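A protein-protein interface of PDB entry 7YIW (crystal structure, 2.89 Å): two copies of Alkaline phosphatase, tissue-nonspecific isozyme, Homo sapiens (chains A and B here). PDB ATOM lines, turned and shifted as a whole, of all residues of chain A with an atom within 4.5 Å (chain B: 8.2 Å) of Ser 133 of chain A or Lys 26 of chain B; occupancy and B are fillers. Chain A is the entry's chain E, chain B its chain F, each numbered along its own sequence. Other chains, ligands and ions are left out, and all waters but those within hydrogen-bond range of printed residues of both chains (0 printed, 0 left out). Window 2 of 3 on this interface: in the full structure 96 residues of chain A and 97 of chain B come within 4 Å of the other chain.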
ATOM      1  N   VAL A 123       5.945 -23.253  14.137  1.00  0.00           N
ATOM      2  CA  VAL A 123       4.681 -22.535  14.211  1.00  0.00           C
ATOM      3  C   VAL A 123       4.632 -21.805  15.545  1.00  0.00           C
ATOM      4  O   VAL A 123       5.030 -22.357  16.577  1.00  0.00           O
ATOM      5  CB  VAL A 123       3.479 -23.492  14.057  1.00  0.00           C
ATOM      6  CG1 VAL A 123       2.187 -22.825  14.506  1.00  0.00           C
ATOM      7  CG2 VAL A 123       3.364 -23.976  12.620  1.00  0.00           C
ATOM      8  N   ALA A 125       2.726 -20.060  18.751  1.00  0.00           N
ATOM      9  CA  ALA A 125       1.597 -20.546  19.529  1.00  0.00           C
ATOM     10  C   ALA A 125       1.364 -19.648  20.735  1.00  0.00           C
ATOM     11  O   ALA A 125       2.127 -18.719  21.010  1.00  0.00           O
ATOM     12  CB  ALA A 125       1.824 -21.990  19.991  1.00  0.00           C
ATOM     13  N   VAL A 132       1.160 -27.298  19.750  1.00  0.00           N
ATOM     14  CA  VAL A 132      -0.141 -27.005  19.162  1.00  0.00           C
ATOM     15  C   VAL A 132      -0.111 -25.603  18.570  1.00  0.00           C
ATOM     16  O   VAL A 132       0.659 -24.742  19.003  1.00  0.00           O
ATOM     17  CB  VAL A 132      -1.295 -27.129  20.185  1.00  0.00           C
ATOM     18  CG1 VAL A 132      -1.516 -28.583  20.579  1.00  0.00           C
ATOM     19  CG2 VAL A 132      -1.018 -26.276  21.406  1.00  0.00           C
ATOM     20  N   SER A 133      -0.958 -25.380  17.568  1.00  0.00           N
ATOM     21  CA  SER A 133      -1.072 -24.068  16.953  1.00  0.00           C
ATOM     22  C   SER A 133      -1.822 -23.114  17.882  1.00  0.00           C
ATOM     23  O   SER A 133      -2.300 -23.488  18.957  1.00  0.00           O
ATOM     24  CB  SER A 133      -1.773 -24.176  15.600  1.00  0.00           C
ATOM     25  OG  SER A 133      -3.183 -24.189  15.750  1.00  0.00           O
ATOM     26  N   ALA A 134      -1.928 -21.854  17.456  1.00  0.00           N
ATOM     27  CA  ALA A 134      -2.635 -20.848  18.241  1.00  0.00           C
ATOM     28  C   ALA A 134      -4.144 -21.043  18.238  1.00  0.00           C
ATOM     29  O   ALA A 134      -4.847 -20.292  18.922  1.00  0.00           O
ATOM     30  CB  ALA A 134      -2.291 -19.449  17.732  1.00  0.00           C
ATOM     31  N   ALA A 135      -4.663 -22.018  17.485  1.00  0.00           N
ATOM     32  CA  ALA A 135      -6.078 -22.353  17.576  1.00  0.00           C
ATOM     33  C   ALA A 135      -6.422 -23.006  18.907  1.00  0.00           C
ATOM     34  O   ALA A 135      -7.587 -22.971  19.319  1.00  0.00           O
ATOM     35  CB  ALA A 135      -6.480 -23.274  16.423  1.00  0.00           C
ATOM     36  N   THR A 136      -5.439 -23.597  19.582  1.00  0.00           N
ATOM     37  CA  THR A 136      -5.660 -24.202  20.887  1.00  0.00           C
ATOM     38  C   THR A 136      -5.676 -23.123  21.964  1.00  0.00           C
ATOM     39  O   THR A 136      -4.789 -22.264  22.006  1.00  0.00           O
ATOM     40  CB  THR A 136      -4.569 -25.232  21.188  1.00  0.00           C
ATOM     41  OG1 THR A 136      -4.681 -26.335  20.279  1.00  0.00           O
ATOM     42  CG2 THR A 136      -4.683 -25.746  22.619  1.00  0.00           C
ATOM     43  N   ASN A 147      -5.194 -29.549  15.837  1.00  0.00           N
ATOM     44  CA  ASN A 147      -4.288 -28.408  15.904  1.00  0.00           C
ATOM     45  C   ASN A 147      -2.887 -28.785  16.374  1.00  0.00           C
ATOM     46  O   ASN A 147      -2.090 -27.890  16.681  1.00  0.00           O
ATOM     47  CB  ASN A 147      -4.871 -27.326  16.819  1.00  0.00           C
ATOM     48  CG  ASN A 147      -6.290 -26.949  16.443  1.00  0.00           C
ATOM     49  OD1 ASN A 147      -6.624 -26.837  15.263  1.00  0.00           O
ATOM     50  ND2 ASN A 147      -7.136 -26.752  17.447  1.00  0.00           N
ATOM     51  N   VAL A 149       0.962 -29.704  16.125  1.00  0.00           N
ATOM     52  CA  VAL A 149       2.069 -29.466  15.208  1.00  0.00           C
ATOM     53  C   VAL A 149       3.260 -30.290  15.675  1.00  0.00           C
ATOM     54  O   VAL A 149       3.507 -30.415  16.880  1.00  0.00           O
ATOM     55  CB  VAL A 149       2.428 -27.965  15.108  1.00  0.00           C
ATOM     56  CG1 VAL A 149       1.259 -27.177  14.534  1.00  0.00           C
ATOM     57  CG2 VAL A 149       2.827 -27.409  16.466  1.00  0.00           C
ATOM     58  N   LEU B  20      -5.136 -10.909  22.171  1.00  0.00           N
ATOM     59  CA  LEU B  20      -5.734 -10.439  20.924  1.00  0.00           C
ATOM     60  C   LEU B  20      -5.813 -11.563  19.897  1.00  0.00           C
ATOM     61  O   LEU B  20      -6.902 -12.033  19.562  1.00  0.00           O
ATOM     62  CB  LEU B  20      -4.936  -9.265  20.352  1.00  0.00           C
ATOM     63  CG  LEU B  20      -5.421  -7.868  20.739  1.00  0.00           C
ATOM     64  CD1 LEU B  20      -4.296  -6.854  20.609  1.00  0.00           C
ATOM     65  CD2 LEU B  20      -6.621  -7.458  19.898  1.00  0.00           C
ATOM     66  N   VAL B  21      -4.646 -11.968  19.404  1.00  0.00           N
ATOM     67  CA  VAL B  21      -4.489 -13.085  18.472  1.00  0.00           C
ATOM     68  C   VAL B  21      -5.145 -12.760  17.134  1.00  0.00           C
ATOM     69  O   VAL B  21      -6.361 -12.949  16.977  1.00  0.00           O
ATOM     70  CB  VAL B  21      -5.054 -14.390  19.057  1.00  0.00           C
ATOM     71  CG1 VAL B  21      -4.819 -15.535  18.097  1.00  0.00           C
ATOM     72  CG2 VAL B  21      -4.426 -14.688  20.414  1.00  0.00           C
ATOM     73  N   PRO B  22      -4.390 -12.265  16.153  1.00  0.00           N
ATOM     74  CA  PRO B  22      -4.948 -12.112  14.805  1.00  0.00           C
ATOM     75  C   PRO B  22      -5.405 -13.453  14.250  1.00  0.00           C
ATOM     76  O   PRO B  22      -4.813 -14.499  14.525  1.00  0.00           O
ATOM     77  CB  PRO B  22      -3.779 -11.540  13.992  1.00  0.00           C
ATOM     78  CG  PRO B  22      -2.853 -10.946  14.995  1.00  0.00           C
ATOM     79  CD  PRO B  22      -3.034 -11.705  16.274  1.00  0.00           C
ATOM     80  N   GLU B  23      -6.482 -13.409  13.463  1.00  0.00           N
ATOM     81  CA  GLU B  23      -7.067 -14.638  12.936  1.00  0.00           C
ATOM     82  C   GLU B  23      -6.082 -15.396  12.054  1.00  0.00           C
ATOM     83  O   GLU B  23      -6.049 -16.632  12.068  1.00  0.00           O
ATOM     84  CB  GLU B  23      -8.344 -14.315  12.162  1.00  0.00           C
ATOM     85  CG  GLU B  23      -9.204 -15.526  11.799  1.00  0.00           C
ATOM     86  CD  GLU B  23      -9.719 -16.300  13.002  1.00  0.00           C
ATOM     87  OE1 GLU B  23      -9.668 -15.771  14.134  1.00  0.00           O
ATOM     88  OE2 GLU B  23     -10.184 -17.446  12.808  1.00  0.00           O
ATOM     89  N   LYS B  24      -5.268 -14.673  11.282  1.00  0.00           N
ATOM     90  CA  LYS B  24      -4.327 -15.324  10.377  1.00  0.00           C
ATOM     91  C   LYS B  24      -3.220 -16.067  11.115  1.00  0.00           C
ATOM     92  O   LYS B  24      -2.648 -17.008  10.559  1.00  0.00           O
ATOM     93  CB  LYS B  24      -3.718 -14.298   9.418  1.00  0.00           C
ATOM     94  CG  LYS B  24      -2.705 -13.360  10.052  1.00  0.00           C
ATOM     95  CD  LYS B  24      -2.137 -12.392   9.028  1.00  0.00           C
ATOM     96  CE  LYS B  24      -1.021 -11.552   9.626  1.00  0.00           C
ATOM     97  NZ  LYS B  24      -0.455 -10.594   8.638  1.00  0.00           N
ATOM     98  N   GLU B  25      -2.910 -15.676  12.351  1.00  0.00           N
ATOM     99  CA  GLU B  25      -1.831 -16.316  13.091  1.00  0.00           C
ATOM    100  C   GLU B  25      -2.265 -17.596  13.792  1.00  0.00           C
ATOM    101  O   GLU B  25      -1.404 -18.339  14.275  1.00  0.00           O
ATOM    102  CB  GLU B  25      -1.241 -15.333  14.105  1.00  0.00           C
ATOM    103  CG  GLU B  25      -0.594 -14.116  13.458  1.00  0.00           C
ATOM    104  CD  GLU B  25       0.148 -13.241  14.452  1.00  0.00           C
ATOM    105  OE1 GLU B  25       0.127 -13.560  15.659  1.00  0.00           O
ATOM    106  OE2 GLU B  25       0.753 -12.234  14.022  1.00  0.00           O
ATOM    107  N   LYS B  26      -3.569 -17.873  13.856  1.00  0.00           N
ATOM    108  CA  LYS B  26      -4.054 -19.143  14.379  1.00  0.00           C
ATOM    109  C   LYS B  26      -3.864 -20.292  13.398  1.00  0.00           C
ATOM    110  O   LYS B  26      -4.047 -21.451  13.784  1.00  0.00           O
ATOM    111  CB  LYS B  26      -5.538 -19.041  14.742  1.00  0.00           C
ATOM    112  CG  LYS B  26      -5.846 -18.188  15.958  1.00  0.00           C
ATOM    113  CD  LYS B  26      -7.307 -18.336  16.356  1.00  0.00           C
ATOM    114  CE  LYS B  26      -7.801 -17.140  17.156  1.00  0.00           C
ATOM    115  NZ  LYS B  26      -9.159 -16.696  16.730  1.00  0.00           N
ATOM    116  N   ASP B  27      -3.505 -19.996  12.149  1.00  0.00           N
ATOM    117  CA  ASP B  27      -3.375 -21.009  11.112  1.00  0.00           C
ATOM    118  C   ASP B  27      -1.911 -21.381  10.959  1.00  0.00           C
ATOM    119  O   ASP B  27      -1.091 -20.499  10.655  1.00  0.00           O
ATOM    120  CB  ASP B  27      -3.932 -20.481   9.793  1.00  0.00           C
ATOM    121  CG  ASP B  27      -3.875 -21.503   8.672  1.00  0.00           C
ATOM    122  OD1 ASP B  27      -3.698 -22.707   8.954  1.00  0.00           O
ATOM    123  OD2 ASP B  27      -4.012 -21.096   7.499  1.00  0.00           O
ATOM    124  N   PRO B  28      -1.531 -22.647  11.162  1.00  0.00           N
ATOM    125  CA  PRO B  28      -0.111 -23.013  11.035  1.00  0.00           C
ATOM    126  C   PRO B  28       0.474 -22.711   9.670  1.00  0.00           C
ATOM    127  O   PRO B  28       1.661 -22.375   9.580  1.00  0.00           O
ATOM    128  CB  PRO B  28      -0.109 -24.521  11.325  1.00  0.00           C
ATOM    129  CG  PRO B  28      -1.360 -24.767  12.092  1.00  0.00           C
ATOM    130  CD  PRO B  28      -2.365 -23.790  11.569  1.00  0.00           C
ATOM    131  N   LYS B  29      -0.326 -22.811   8.604  1.00  0.00           N
ATOM    132  CA  LYS B  29       0.184 -22.546   7.263  1.00  0.00           C
ATOM    133  C   LYS B  29       0.716 -21.124   7.134  1.00  0.00           C
ATOM    134  O   LYS B  29       1.639 -20.879   6.350  1.00  0.00           O
ATOM    135  CB  LYS B  29      -0.909 -22.804   6.223  1.00  0.00           C
ATOM    136  CG  LYS B  29      -0.418 -22.805   4.780  1.00  0.00           C
ATOM    137  CD  LYS B  29      -1.588 -22.831   3.804  1.00  0.00           C
ATOM    138  CE  LYS B  29      -1.124 -22.986   2.363  1.00  0.00           C
ATOM    139  NZ  LYS B  29       0.290 -23.442   2.264  1.00  0.00           N
ATOM    140  N   TYR B  30       0.158 -20.181   7.895  1.00  0.00           N
ATOM    141  CA  TYR B  30       0.659 -18.810   7.862  1.00  0.00           C
ATOM    142  C   TYR B  30       2.102 -18.744   8.343  1.00  0.00           C
ATOM    143  O   TYR B  30       2.953 -18.113   7.706  1.00  0.00           O
ATOM    144  CB  TYR B  30      -0.234 -17.904   8.711  1.00  0.00           C
ATOM    145  CG  TYR B  30       0.384 -16.562   9.044  1.00  0.00           C
ATOM    146  CD1 TYR B  30       0.310 -15.503   8.149  1.00  0.00           C
ATOM    147  CD2 TYR B  30       1.032 -16.351  10.258  1.00  0.00           C
ATOM    148  CE1 TYR B  30       0.872 -14.275   8.446  1.00  0.00           C
ATOM    149  CE2 TYR B  30       1.596 -15.127  10.564  1.00  0.00           C
ATOM    150  CZ  TYR B  30       1.512 -14.092   9.655  1.00  0.00           C
ATOM    151  OH  TYR B  30       2.071 -12.871   9.955  1.00  0.00           O
ATOM    152  N   TRP B  31       2.395 -19.392   9.473  1.00  0.00           N
ATOM    153  CA  TRP B  31       3.747 -19.354  10.017  1.00  0.00           C
ATOM    154  C   TRP B  31       4.719 -20.172   9.178  1.00  0.00           C
ATOM    155  O   TRP B  31       5.906 -19.835   9.105  1.00  0.00           O
ATOM    156  CB  TRP B  31       3.744 -19.841  11.466  1.00  0.00           C
ATOM    157  CG  TRP B  31       3.008 -18.918  12.385  1.00  0.00           C
ATOM    158  CD1 TRP B  31       1.779 -19.121  12.942  1.00  0.00           C
ATOM    159  CD2 TRP B  31       3.450 -17.634  12.842  1.00  0.00           C
ATOM    160  NE1 TRP B  31       1.430 -18.046  13.723  1.00  0.00           N
ATOM    161  CE2 TRP B  31       2.440 -17.119  13.678  1.00  0.00           C
ATOM    162  CE3 TRP B  31       4.602 -16.871  12.626  1.00  0.00           C
ATOM    163  CZ2 TRP B  31       2.548 -15.877  14.301  1.00  0.00           C
ATOM    164  CZ3 TRP B  31       4.706 -15.639  13.244  1.00  0.00           C
ATOM    165  CH2 TRP B  31       3.686 -15.154  14.071  1.00  0.00           C
ATOM    166  N   ARG B  32       4.240 -21.241   8.537  1.00  0.00           N
ATOM    167  CA  ARG B  32       5.097 -22.011   7.639  1.00  0.00           C
ATOM    168  C   ARG B  32       5.324 -21.280   6.321  1.00  0.00           C
ATOM    169  O   ARG B  32       6.444 -21.278   5.799  1.00  0.00           O
ATOM    170  CB  ARG B  32       4.499 -23.396   7.391  1.00  0.00           C
ATOM    171  CG  ARG B  32       4.049 -24.102   8.657  1.00  0.00           C
ATOM    172  CD  ARG B  32       4.090 -25.613   8.515  1.00  0.00           C
ATOM    173  NE  ARG B  32       3.864 -26.280   9.791  1.00  0.00           N
ATOM    174  CZ  ARG B  32       2.879 -27.135  10.026  1.00  0.00           C
ATOM    175  NH1 ARG B  32       2.005 -27.459   9.085  1.00  0.00           N
ATOM    176  NH2 ARG B  32       2.766 -27.682  11.233  1.00  0.00           N
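O of Lys 26 of chain B is in hydrogen-bond range of OG of Ser 133 of chain A, at 3.5 Å.
The side-chain amino group (NZ) of Lys 26 of chain B is in salt-bridge range of the side-chain carboxylate (OE1) of Glu 23 of chain B (2.8 Å). O of Glu 25 of chain B sits at hydrogen-bond distance from NE1 of Trp 31 of chain B. The side-chain hydroxyl (OG) of Ser 133 of chain A lies close to the backbone NH (N) of Ala 135 of chain A, at 3.1 Å. The backbone NH (N) of Ser 133 of chain A sits at hydrogen-bond distance from the backbone carbonyl oxygen (O) of Asn 147 of chain A, 2.9 Å away.
CG2 of Val 123 of chain A touches CB of Pro 28 of chain B (3.7 Å). CA of Val 123 of chain A touches CB of Trp 31 of chain B (3.96 Å). NE of Arg 32 of chain B touches CG2 of Val 123 of chain A, at 3.7 Å. Pro 28 of chain B touches Ser 133 of chain A (CG to CB, 3.6 Å). Ala 134 of chain A touches Glu 25 of chain B. O of Ala 134 of chain A touches CG of Lys 26 of chain B, at 3.8 Å. Ala 135 of chain A touches Lys 26 of chain B (N to O, 3.8 Å). Arg 32 of chain B touches Val 149 of chain A.
Printed residues of chain B within 4 Å of Val 123 of chain A: Pro 28 (3.7 Å), Trp 31 (3.96 Å) and Arg 32 (3.7 Å). Ala 125 of chain A touches none of the printed residues of chain B. Of chain B, only Glu 25 and Lys 26 come within 4 Å of Ala 134 of chain A. Printed residues of chain B within 4 Å of Ala 135 of chain A: Lys 26. Printed residues of chain B within 4 Å of Val 149 of chain A: Arg 32 (3.7 Å). Lys 26 of chain B touches three residues of chain A. Of the printed residues of chain A, Trp 31 of chain B touches Val 123 (3.96 Å). The nearest printed residue of chain A that does not touch Lys 26 of chain B is Asn 147 of chain A (6.2 Å).
Hydrophobic or aromatic side chains of chain A within 4 Å of the printed part of chain B: Val 123, Ala 134 and Val 149. Among the printed residues, no Asp or Glu carboxylate lies within 4 Å of a Lys or Arg side-chain nitrogen of the other chain.
No position is printed for both chains. Of the 9 pairs that touch across the chains among the printed residues, none has its exchanged pair printed and touching as well.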
